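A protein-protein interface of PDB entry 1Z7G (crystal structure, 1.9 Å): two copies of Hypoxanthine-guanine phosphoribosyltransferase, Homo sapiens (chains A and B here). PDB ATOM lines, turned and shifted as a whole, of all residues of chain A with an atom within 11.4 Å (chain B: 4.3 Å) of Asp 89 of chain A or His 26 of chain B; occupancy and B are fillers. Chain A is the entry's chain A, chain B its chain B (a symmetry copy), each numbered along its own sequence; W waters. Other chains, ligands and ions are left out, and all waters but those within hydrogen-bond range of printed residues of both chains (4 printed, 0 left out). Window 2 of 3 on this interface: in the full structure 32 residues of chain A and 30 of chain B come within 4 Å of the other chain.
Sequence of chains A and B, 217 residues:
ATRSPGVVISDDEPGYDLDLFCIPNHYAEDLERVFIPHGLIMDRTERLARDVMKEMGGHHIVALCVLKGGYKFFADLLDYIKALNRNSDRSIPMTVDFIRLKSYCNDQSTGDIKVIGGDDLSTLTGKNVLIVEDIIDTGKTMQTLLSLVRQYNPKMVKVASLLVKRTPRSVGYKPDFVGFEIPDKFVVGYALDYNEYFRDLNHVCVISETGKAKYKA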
ATOM      1  N   MET A  53     -21.830 -14.117  -4.337  1.00  0.00           N
ATOM      2  CA  MET A  53     -21.303 -12.835  -3.887  1.00  0.00           C
ATOM      3  C   MET A  53     -20.562 -12.102  -4.991  1.00  0.00           C
ATOM      4  O   MET A  53     -20.569 -10.871  -5.042  1.00  0.00           O
ATOM      5  CB  MET A  53     -20.387 -13.037  -2.684  1.00  0.00           C
ATOM      6  CG  MET A  53     -21.142 -13.390  -1.418  1.00  0.00           C
ATOM      7  SD  MET A  53     -22.330 -12.098  -0.955  1.00  0.00           S
ATOM      8  CE  MET A  53     -21.302 -11.094   0.104  1.00  0.00           C
ATOM      9  N   GLY A  57     -23.004  -9.640  -4.834  1.00  0.00           N
ATOM     10  CA  GLY A  57     -22.491  -8.946  -3.665  1.00  0.00           C
ATOM     11  C   GLY A  57     -22.384  -7.438  -3.844  1.00  0.00           C
ATOM     12  O   GLY A  57     -22.611  -6.909  -4.933  1.00  0.00           O
ATOM     13  N   GLY A  58     -22.041  -6.739  -2.767  1.00  0.00           N
ATOM     14  CA  GLY A  58     -21.904  -5.294  -2.841  1.00  0.00           C
ATOM     15  C   GLY A  58     -23.224  -4.551  -2.771  1.00  0.00           C
ATOM     16  O   GLY A  58     -23.244  -3.336  -2.593  1.00  0.00           O
ATOM     17  N   HIS A  59     -24.326  -5.279  -2.913  1.00  0.00           N
ATOM     18  CA  HIS A  59     -25.654  -4.682  -2.859  1.00  0.00           C
ATOM     19  C   HIS A  59     -26.541  -5.519  -1.941  1.00  0.00           C
ATOM     20  O   HIS A  59     -26.176  -6.635  -1.556  1.00  0.00           O
ATOM     21  CB  HIS A  59     -26.272  -4.621  -4.261  1.00  0.00           C
ATOM     22  CG  HIS A  59     -25.385  -3.990  -5.292  1.00  0.00           C
ATOM     23  ND1 HIS A  59     -24.908  -2.702  -5.178  1.00  0.00           N
ATOM     24  CD2 HIS A  59     -24.905  -4.466  -6.465  1.00  0.00           C
ATOM     25  CE1 HIS A  59     -24.173  -2.411  -6.237  1.00  0.00           C
ATOM     26  NE2 HIS A  59     -24.156  -3.464  -7.034  1.00  0.00           N
ATOM     27  N   ILE A  81     -22.238 -17.510   2.750  1.00  0.00           N
ATOM     28  CA  ILE A  81     -22.414 -16.176   2.190  1.00  0.00           C
ATOM     29  C   ILE A  81     -22.110 -15.155   3.271  1.00  0.00           C
ATOM     30  O   ILE A  81     -21.390 -14.189   3.039  1.00  0.00           O
ATOM     31  CB  ILE A  81     -23.858 -15.944   1.693  1.00  0.00           C
ATOM     32  CG1 ILE A  81     -24.083 -16.684   0.373  1.00  0.00           C
ATOM     33  CG2 ILE A  81     -24.128 -14.447   1.536  1.00  0.00           C
ATOM     34  CD1 ILE A  81     -23.233 -16.172  -0.759  1.00  0.00           C
ATOM     35  N   LYS A  82     -22.669 -15.376   4.455  1.00  0.00           N
ATOM     36  CA  LYS A  82     -22.447 -14.463   5.569  1.00  0.00           C
ATOM     37  C   LYS A  82     -20.974 -14.414   5.975  1.00  0.00           C
ATOM     38  O   LYS A  82     -20.465 -13.356   6.340  1.00  0.00           O
ATOM     39  CB  LYS A  82     -23.334 -14.866   6.748  1.00  0.00           C
ATOM     40  CG  LYS A  82     -24.750 -14.346   6.605  1.00  0.00           C
ATOM     41  CD  LYS A  82     -25.781 -15.289   7.209  1.00  0.00           C
ATOM     42  CE  LYS A  82     -25.538 -15.546   8.681  1.00  0.00           C
ATOM     43  NZ  LYS A  82     -26.719 -16.222   9.306  1.00  0.00           N
ATOM     44  N   ALA A  83     -20.282 -15.546   5.889  1.00  0.00           N
ATOM     45  CA  ALA A  83     -18.866 -15.579   6.249  1.00  0.00           C
ATOM     46  C   ALA A  83     -18.056 -14.666   5.329  1.00  0.00           C
ATOM     47  O   ALA A  83     -17.059 -14.084   5.752  1.00  0.00           O
ATOM     48  CB  ALA A  83     -18.329 -17.012   6.186  1.00  0.00           C
ATOM     49  N   LEU A  84     -18.487 -14.541   4.074  1.00  0.00           N
ATOM     50  CA  LEU A  84     -17.809 -13.678   3.108  1.00  0.00           C
ATOM     51  C   LEU A  84     -18.179 -12.218   3.347  1.00  0.00           C
ATOM     52  O   LEU A  84     -17.339 -11.329   3.254  1.00  0.00           O
ATOM     53  CB  LEU A  84     -18.207 -14.062   1.681  1.00  0.00           C
ATOM     54  CG  LEU A  84     -17.682 -15.393   1.152  1.00  0.00           C
ATOM     55  CD1 LEU A  84     -18.381 -15.732  -0.161  1.00  0.00           C
ATOM     56  CD2 LEU A  84     -16.171 -15.288   0.947  1.00  0.00           C
ATOM     57  N   ASN A  85     -19.452 -11.986   3.642  1.00  0.00           N
ATOM     58  CA  ASN A  85     -19.969 -10.648   3.901  1.00  0.00           C
ATOM     59  C   ASN A  85     -19.226  -9.995   5.072  1.00  0.00           C
ATOM     60  O   ASN A  85     -19.126  -8.773   5.148  1.00  0.00           O
ATOM     61  CB  ASN A  85     -21.471 -10.738   4.197  1.00  0.00           C
ATOM     62  CG  ASN A  85     -22.071  -9.415   4.625  1.00  0.00           C
ATOM     63  OD1 ASN A  85     -21.804  -8.924   5.722  1.00  0.00           O
ATOM     64  ND2 ASN A  85     -22.892  -8.831   3.761  1.00  0.00           N
ATOM     65  N   ARG A  86     -18.698 -10.819   5.973  1.00  0.00           N
ATOM     66  CA  ARG A  86     -17.974 -10.327   7.147  1.00  0.00           C
ATOM     67  C   ARG A  86     -16.688  -9.558   6.861  1.00  0.00           C
ATOM     68  O   ARG A  86     -16.338  -8.635   7.599  1.00  0.00           O
ATOM     69  CB  ARG A  86     -17.656 -11.493   8.084  1.00  0.00           C
ATOM     70  CG  ARG A  86     -18.895 -12.085   8.696  1.00  0.00           C
ATOM     71  CD  ARG A  86     -18.662 -13.454   9.299  1.00  0.00           C
ATOM     72  NE  ARG A  86     -19.954 -14.083   9.532  1.00  0.00           N
ATOM     73  CZ  ARG A  86     -20.139 -15.369   9.787  1.00  0.00           C
ATOM     74  NH1 ARG A  86     -19.105 -16.202   9.854  1.00  0.00           N
ATOM     75  NH2 ARG A  86     -21.370 -15.822   9.955  1.00  0.00           N
ATOM     76  N   ASN A  87     -15.986  -9.936   5.797  1.00  0.00           N
ATOM     77  CA  ASN A  87     -14.726  -9.291   5.455  1.00  0.00           C
ATOM     78  C   ASN A  87     -14.903  -8.005   4.659  1.00  0.00           C
ATOM     79  O   ASN A  87     -13.929  -7.316   4.377  1.00  0.00           O
ATOM     80  CB  ASN A  87     -13.836 -10.262   4.672  1.00  0.00           C
ATOM     81  CG  ASN A  87     -13.645 -11.591   5.390  1.00  0.00           C
ATOM     82  OD1 ASN A  87     -13.351 -11.626   6.583  1.00  0.00           O
ATOM     83  ND2 ASN A  87     -13.807 -12.691   4.660  1.00  0.00           N
ATOM     84  N   SER A  88     -16.144  -7.683   4.308  1.00  0.00           N
ATOM     85  CA  SER A  88     -16.446  -6.478   3.537  1.00  0.00           C
ATOM     86  C   SER A  88     -16.074  -5.201   4.291  1.00  0.00           C
ATOM     87  O   SER A  88     -16.346  -5.082   5.483  1.00  0.00           O
ATOM     88  CB  SER A  88     -17.942  -6.456   3.200  1.00  0.00           C
ATOM     89  OG  SER A  88     -18.272  -5.327   2.417  1.00  0.00           O
ATOM     90  N   ASP A  89     -15.458  -4.241   3.604  1.00  0.00           N
ATOM     91  CA  ASP A  89     -15.082  -2.986   4.261  1.00  0.00           C
ATOM     92  C   ASP A  89     -16.326  -2.210   4.695  1.00  0.00           C
ATOM     93  O   ASP A  89     -16.327  -1.540   5.726  1.00  0.00           O
ATOM     94  CB  ASP A  89     -14.226  -2.114   3.337  1.00  0.00           C
ATOM     95  CG  ASP A  89     -12.838  -2.693   3.097  1.00  0.00           C
ATOM     96  OD1 ASP A  89     -12.371  -3.495   3.937  1.00  0.00           O
ATOM     97  OD2 ASP A  89     -12.207  -2.331   2.075  1.00  0.00           O
ATOM     98  N   ARG A  90     -17.389  -2.304   3.905  1.00  0.00           N
ATOM     99  CA  ARG A  90     -18.632  -1.620   4.224  1.00  0.00           C
ATOM    100  C   ARG A  90     -19.669  -2.655   4.644  1.00  0.00           C
ATOM    101  O   ARG A  90     -19.692  -3.763   4.121  1.00  0.00           O
ATOM    102  CB  ARG A  90     -19.146  -0.830   3.007  1.00  0.00           C
ATOM    103  CG  ARG A  90     -20.332   0.065   3.328  1.00  0.00           C
ATOM    104  CD  ARG A  90     -20.793   0.926   2.144  1.00  0.00           C
ATOM    105  NE  ARG A  90     -19.810   1.935   1.746  1.00  0.00           N
ATOM    106  CZ  ARG A  90     -18.909   1.760   0.785  1.00  0.00           C
ATOM    107  NH1 ARG A  90     -18.866   0.614   0.118  1.00  0.00           N
ATOM    108  NH2 ARG A  90     -18.046   2.723   0.490  1.00  0.00           N
ATOM    109  N   SER A  91     -20.514  -2.298   5.604  1.00  0.00           N
ATOM    110  CA  SER A  91     -21.551  -3.210   6.061  1.00  0.00           C
ATOM    111  C   SER A  91     -22.618  -3.277   4.973  1.00  0.00           C
ATOM    112  O   SER A  91     -23.142  -2.253   4.545  1.00  0.00           O
ATOM    113  CB  SER A  91     -22.189  -2.700   7.352  1.00  0.00           C
ATOM    114  OG  SER A  91     -21.232  -2.573   8.390  1.00  0.00           O
ATOM    115  N   ILE A  92     -22.937  -4.483   4.529  1.00  0.00           N
ATOM    116  CA  ILE A  92     -23.945  -4.657   3.495  1.00  0.00           C
ATOM    117  C   ILE A  92     -25.087  -5.474   4.065  1.00  0.00           C
ATOM    118  O   ILE A  92     -24.886  -6.597   4.529  1.00  0.00           O
ATOM    119  CB  ILE A  92     -23.357  -5.364   2.250  1.00  0.00           C
ATOM    120  CG1 ILE A  92     -22.181  -4.543   1.709  1.00  0.00           C
ATOM    121  CG2 ILE A  92     -24.426  -5.500   1.164  1.00  0.00           C
ATOM    122  CD1 ILE A  92     -21.414  -5.213   0.599  1.00  0.00           C
ATOM    123  N   PRO A  93     -26.305  -4.911   4.052  1.00  0.00           N
ATOM    124  CA  PRO A  93     -27.481  -5.602   4.576  1.00  0.00           C
ATOM    125  C   PRO A  93     -27.871  -6.789   3.709  1.00  0.00           C
ATOM    126  O   PRO A  93     -27.517  -6.857   2.531  1.00  0.00           O
ATOM    127  CB  PRO A  93     -28.544  -4.509   4.573  1.00  0.00           C
ATOM    128  CG  PRO A  93     -28.199  -3.737   3.356  1.00  0.00           C
ATOM    129  CD  PRO A  93     -26.687  -3.609   3.470  1.00  0.00           C
ATOM    130  N   MET A  94     -28.602  -7.720   4.306  1.00  0.00           N
ATOM    131  CA  MET A  94     -29.048  -8.906   3.600  1.00  0.00           C
ATOM    132  C   MET A  94     -30.339  -9.381   4.247  1.00  0.00           C
ATOM    133  O   MET A  94     -30.463  -9.388   5.471  1.00  0.00           O
ATOM    134  CB  MET A  94     -27.984 -10.000   3.681  1.00  0.00           C
ATOM    135  CG  MET A  94     -28.310 -11.238   2.871  1.00  0.00           C
ATOM    136  SD  MET A  94     -27.091 -12.539   3.120  1.00  0.00           S
ATOM    137  CE  MET A  94     -27.761 -13.337   4.563  1.00  0.00           C
ATOM    138  N   PRO B  24     -16.724  -8.589  12.965  1.00  0.00           N
ATOM    139  CA  PRO B  24     -16.493  -8.045  11.621  1.00  0.00           C
ATOM    140  C   PRO B  24     -15.986  -6.609  11.765  1.00  0.00           C
ATOM    141  O   PRO B  24     -16.541  -5.840  12.554  1.00  0.00           O
ATOM    142  CB  PRO B  24     -17.881  -8.096  10.977  1.00  0.00           C
ATOM    143  CG  PRO B  24     -18.561  -9.246  11.696  1.00  0.00           C
ATOM    144  CD  PRO B  24     -18.123  -9.030  13.131  1.00  0.00           C
ATOM    145  N   ASN B  25     -14.944  -6.248  11.018  1.00  0.00           N
ATOM    146  CA  ASN B  25     -14.406  -4.895  11.111  1.00  0.00           C
ATOM    147  C   ASN B  25     -15.472  -3.831  10.916  1.00  0.00           C
ATOM    148  O   ASN B  25     -15.499  -2.843  11.658  1.00  0.00           O
ATOM    149  CB  ASN B  25     -13.307  -4.646  10.068  1.00  0.00           C
ATOM    150  CG  ASN B  25     -12.061  -5.468  10.305  1.00  0.00           C
ATOM    151  OD1 ASN B  25     -11.663  -5.705  11.445  1.00  0.00           O
ATOM    152  ND2 ASN B  25     -11.421  -5.893   9.219  1.00  0.00           N
ATOM    153  N   HIS B  26     -16.349  -4.022   9.927  1.00  0.00           N
ATOM    154  CA  HIS B  26     -17.369  -3.018   9.653  1.00  0.00           C
ATOM    155  C   HIS B  26     -18.386  -2.740  10.762  1.00  0.00           C
ATOM    156  O   HIS B  26     -19.201  -1.827  10.626  1.00  0.00           O
ATOM    157  CB  HIS B  26     -18.087  -3.312   8.315  1.00  0.00           C
ATOM    158  CG  HIS B  26     -18.622  -4.705   8.183  1.00  0.00           C
ATOM    159  ND1 HIS B  26     -19.504  -5.253   9.089  1.00  0.00           N
ATOM    160  CD2 HIS B  26     -18.457  -5.634   7.210  1.00  0.00           C
ATOM    161  CE1 HIS B  26     -19.861  -6.458   8.678  1.00  0.00           C
ATOM    162  NE2 HIS B  26     -19.239  -6.713   7.540  1.00  0.00           N
ATOM    163  N   TYR B  27     -18.340  -3.504  11.856  1.00  0.00           N
ATOM    164  CA  TYR B  27     -19.253  -3.286  12.994  1.00  0.00           C
ATOM    165  C   TYR B  27     -18.510  -2.757  14.227  1.00  0.00           C
ATOM    166  O   TYR B  27     -19.098  -2.628  15.302  1.00  0.00           O
ATOM    167  CB  TYR B  27     -19.962  -4.589  13.393  1.00  0.00           C
ATOM    168  CG  TYR B  27     -20.972  -5.079  12.382  1.00  0.00           C
ATOM    169  CD1 TYR B  27     -21.097  -6.444  12.096  1.00  0.00           C
ATOM    170  CD2 TYR B  27     -21.781  -4.181  11.691  1.00  0.00           C
ATOM    171  CE1 TYR B  27     -22.005  -6.898  11.140  1.00  0.00           C
ATOM    172  CE2 TYR B  27     -22.688  -4.620  10.737  1.00  0.00           C
ATOM    173  CZ  TYR B  27     -22.793  -5.980  10.462  1.00  0.00           C
ATOM    174  OH  TYR B  27     -23.654  -6.411   9.482  1.00  0.00           O
ATOM    175  N   ALA B  28     -17.225  -2.458  14.056  1.00  0.00           N
ATOM    176  CA  ALA B  28     -16.370  -1.976  15.144  1.00  0.00           C
ATOM    177  C   ALA B  28     -16.964  -0.897  16.064  1.00  0.00           C
ATOM    178  O   ALA B  28     -16.799  -0.960  17.284  1.00  0.00           O
ATOM    179  CB  ALA B  28     -15.048  -1.495  14.569  1.00  0.00           C
ATOM    180  N   ASP B  30     -20.291  -0.060  15.924  1.00  0.00           N
ATOM    181  CA  ASP B  30     -21.724  -0.312  15.998  1.00  0.00           C
ATOM    182  C   ASP B  30     -22.184  -1.191  17.150  1.00  0.00           C
ATOM    183  O   ASP B  30     -23.372  -1.431  17.307  1.00  0.00           O
ATOM    184  CB  ASP B  30     -22.188  -0.913  14.670  1.00  0.00           C
ATOM    185  CG  ASP B  30     -21.718  -0.097  13.481  1.00  0.00           C
ATOM    186  OD1 ASP B  30     -21.803   1.149  13.559  1.00  0.00           O
ATOM    187  OD2 ASP B  30     -21.266  -0.693  12.480  1.00  0.00           O
ATOM    188  N   ASP B 200     -24.347 -11.140   9.547  1.00  0.00           N
ATOM    189  CA  ASP B 200     -23.016 -11.718   9.417  1.00  0.00           C
ATOM    190  C   ASP B 200     -22.261 -11.746  10.745  1.00  0.00           C
ATOM    191  O   ASP B 200     -21.144 -12.253  10.819  1.00  0.00           O
ATOM    192  CB  ASP B 200     -22.218 -10.960   8.355  1.00  0.00           C
ATOM    193  CG  ASP B 200     -22.151  -9.474   8.629  1.00  0.00           C
ATOM    194  OD1 ASP B 200     -23.213  -8.811   8.676  1.00  0.00           O
ATOM    195  OD2 ASP B 200     -21.026  -8.972   8.799  1.00  0.00           O
ATOM    196  N   TYR B 215     -27.743   2.205  11.139  1.00  0.00           N
ATOM    197  CA  TYR B 215     -28.566   1.215  10.447  1.00  0.00           C
ATOM    198  C   TYR B 215     -30.074   1.356  10.638  1.00  0.00           C
ATOM    199  O   TYR B 215     -30.839   0.455  10.288  1.00  0.00           O
ATOM    200  CB  TYR B 215     -28.113  -0.188  10.858  1.00  0.00           C
ATOM    201  CG  TYR B 215     -26.629  -0.405  10.667  1.00  0.00           C
ATOM    202  CD1 TYR B 215     -26.024  -0.159   9.435  1.00  0.00           C
ATOM    203  CD2 TYR B 215     -25.825  -0.836  11.721  1.00  0.00           C
ATOM    204  CE1 TYR B 215     -24.657  -0.334   9.255  1.00  0.00           C
ATOM    205  CE2 TYR B 215     -24.456  -1.018  11.551  1.00  0.00           C
ATOM    206  CZ  TYR B 215     -23.878  -0.762  10.314  1.00  0.00           C
ATOM    207  OH  TYR B 215     -22.528  -0.919  10.139  1.00  0.00           O
HETATM  208  O   HOH W   1     -13.656  -8.436   9.444  1.00  0.00           O
HETATM  209  O   HOH W   2     -14.439  -2.437   7.534  1.00  0.00           O
HETATM  210  O   HOH W   3     -15.455  -5.979   7.999  1.00  0.00           O
HETATM  211  O   HOH W   4     -21.575  -6.533   5.023  1.00  0.00           O
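Water W4 lies within hydrogen-bond range of the side-chain amide oxygen of Asn 85 of chain A (2.5 Å), the backbone NH of Ile 92 of chain A (2.5 Å), a ring nitrogen (NE2) of His 26 of chain B (3.4 Å) and the backbone carbonyl oxygen of Arg 90 of chain A (3.5 Å). Water W2 lies within hydrogen-bond range of O of Asp 89 of chain A and N of His 26 of chain B. Water W3 lies within hydrogen-bond range of the backbone carbonyl oxygen (O) of Ser 88 of chain A (2.8 Å), the backbone carbonyl oxygen (O) of Arg 86 of chain A (2.8 Å), the backbone NH (N) of His 26 of chain B (2.9 Å) and the backbone NH (N) of Asn 25 of chain B (3.1 Å). Water W1 bridges the backbone NH of Asn 25 of chain B and the backbone carbonyl oxygen of Arg 86 of chain A.
No position is printed for both chains. Of the 12 pairs that touch across the chains among the printed residues, none has its exchanged pair printed and touching as well.
Asp 89 of chain A touches just one residue of chain B: His 26. Asn 25 of chain B touches none of the printed residues of chain A. Of the printed residues of chain A, Tyr 27 of chain B touches Ser 91 (3.4 Å). No residue of chain A comes within 4 Å of Ala 28 of chain B. Printed residues of chain B within 4 Å of Arg 86 of chain A: Pro 24, His 26 and Asp 200. Of the printed residues of chain A, Tyr 215 of chain B touches Ser 91. Printed residues of chain B within 4 Å of Arg 90 of chain A: His 26 (3.8 Å). Printed residues of chain B within 4 Å of Lys 82 of chain A: Asp 200 (3.6 Å). Of the printed residues of chain B, Ser 91 of chain A touches His 26, Tyr 27 and Tyr 215. Asp 30 of chain B touches none of the printed residues of chain A. The nearest printed residue of chain B that does not touch Asp 89 of chain A is Asn 25 of chain B (5.7 Å). The nearest residue of chain A that does not touch His 26 of chain B is Asn 87 of chain A (4.9 Å).
O of Lys 82 of chain A sits close to NE of Arg 86 of chain A, 3.3 Å away. OG of Ser 88 of chain A lies within hydrogen-bond range of O of Arg 90 of chain A, 2.7 Å away. A ring nitrogen (NE2) of His 26 of chain B sits close to the side-chain carboxylate of Asp 200 of chain B, 3.1 Å away. The backbone carbonyl oxygen of His 26 of chain B lies within hydrogen-bond range of the side-chain hydroxyl of Tyr 215 of chain B (3.5 Å). The side-chain hydroxyl (OH) of Tyr 27 of chain B sits at hydrogen-bond distance from the side-chain carboxylate (OD1) of Asp 200 of chain B (2.6 Å). OD2 of Asp 30 of chain B lies within hydrogen-bond range of OH of Tyr 215 of chain B (2.7 Å).
Printed residues of chain A that touch a printed residue of chain B: Lys 82, Asn 85, Arg 86, Ser 88, Asp 89, Arg 90 and Ser 91. Among the printed residues, no Asp or Glu carboxylate lies within 4 Å of a Lys or Arg side-chain nitrogen of the other chain.
NE2 of His 26 of chain B is in hydrogen-bond range of O of Asn 85 of chain A (3.2 Å). OD1 of Asn 85 of chain A lies close to OD2 of Asp 200 of chain B, at 3.2 Å. O of Arg 86 of chain A lies within hydrogen-bond range of NE2 of His 26 of chain B. O of Asp 200 of chain B sits at hydrogen-bond distance from NE of Arg 86 of chain A (2.5 Å). The side-chain hydroxyl (OG) of Ser 91 of chain A sits at hydrogen-bond distance from the backbone carbonyl oxygen (O) of His 26 of chain B, at 3.1 Å. The side-chain hydroxyl (OG) of Ser 91 of chain A lies within hydrogen-bond range of the side-chain hydroxyl (OH) of Tyr 215 of chain B, at 2.7 Å.
Among the printed residues, merely in contact across the chains: Ser 88 of chain A with His 26 of chain B (2.8 Å), Ser 91 of chain A with Tyr 27 of chain B (3.4 Å), Lys 82 of chain A with Asp 200 of chain B (3.6 Å), Asp 89 of chain A with His 26 of chain B (3.6 Å), Arg 86 of chain A with Pro 24 of chain B (3.8 Å) and Arg 90 of chain A with His 26 of chain B (3.8 Å).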
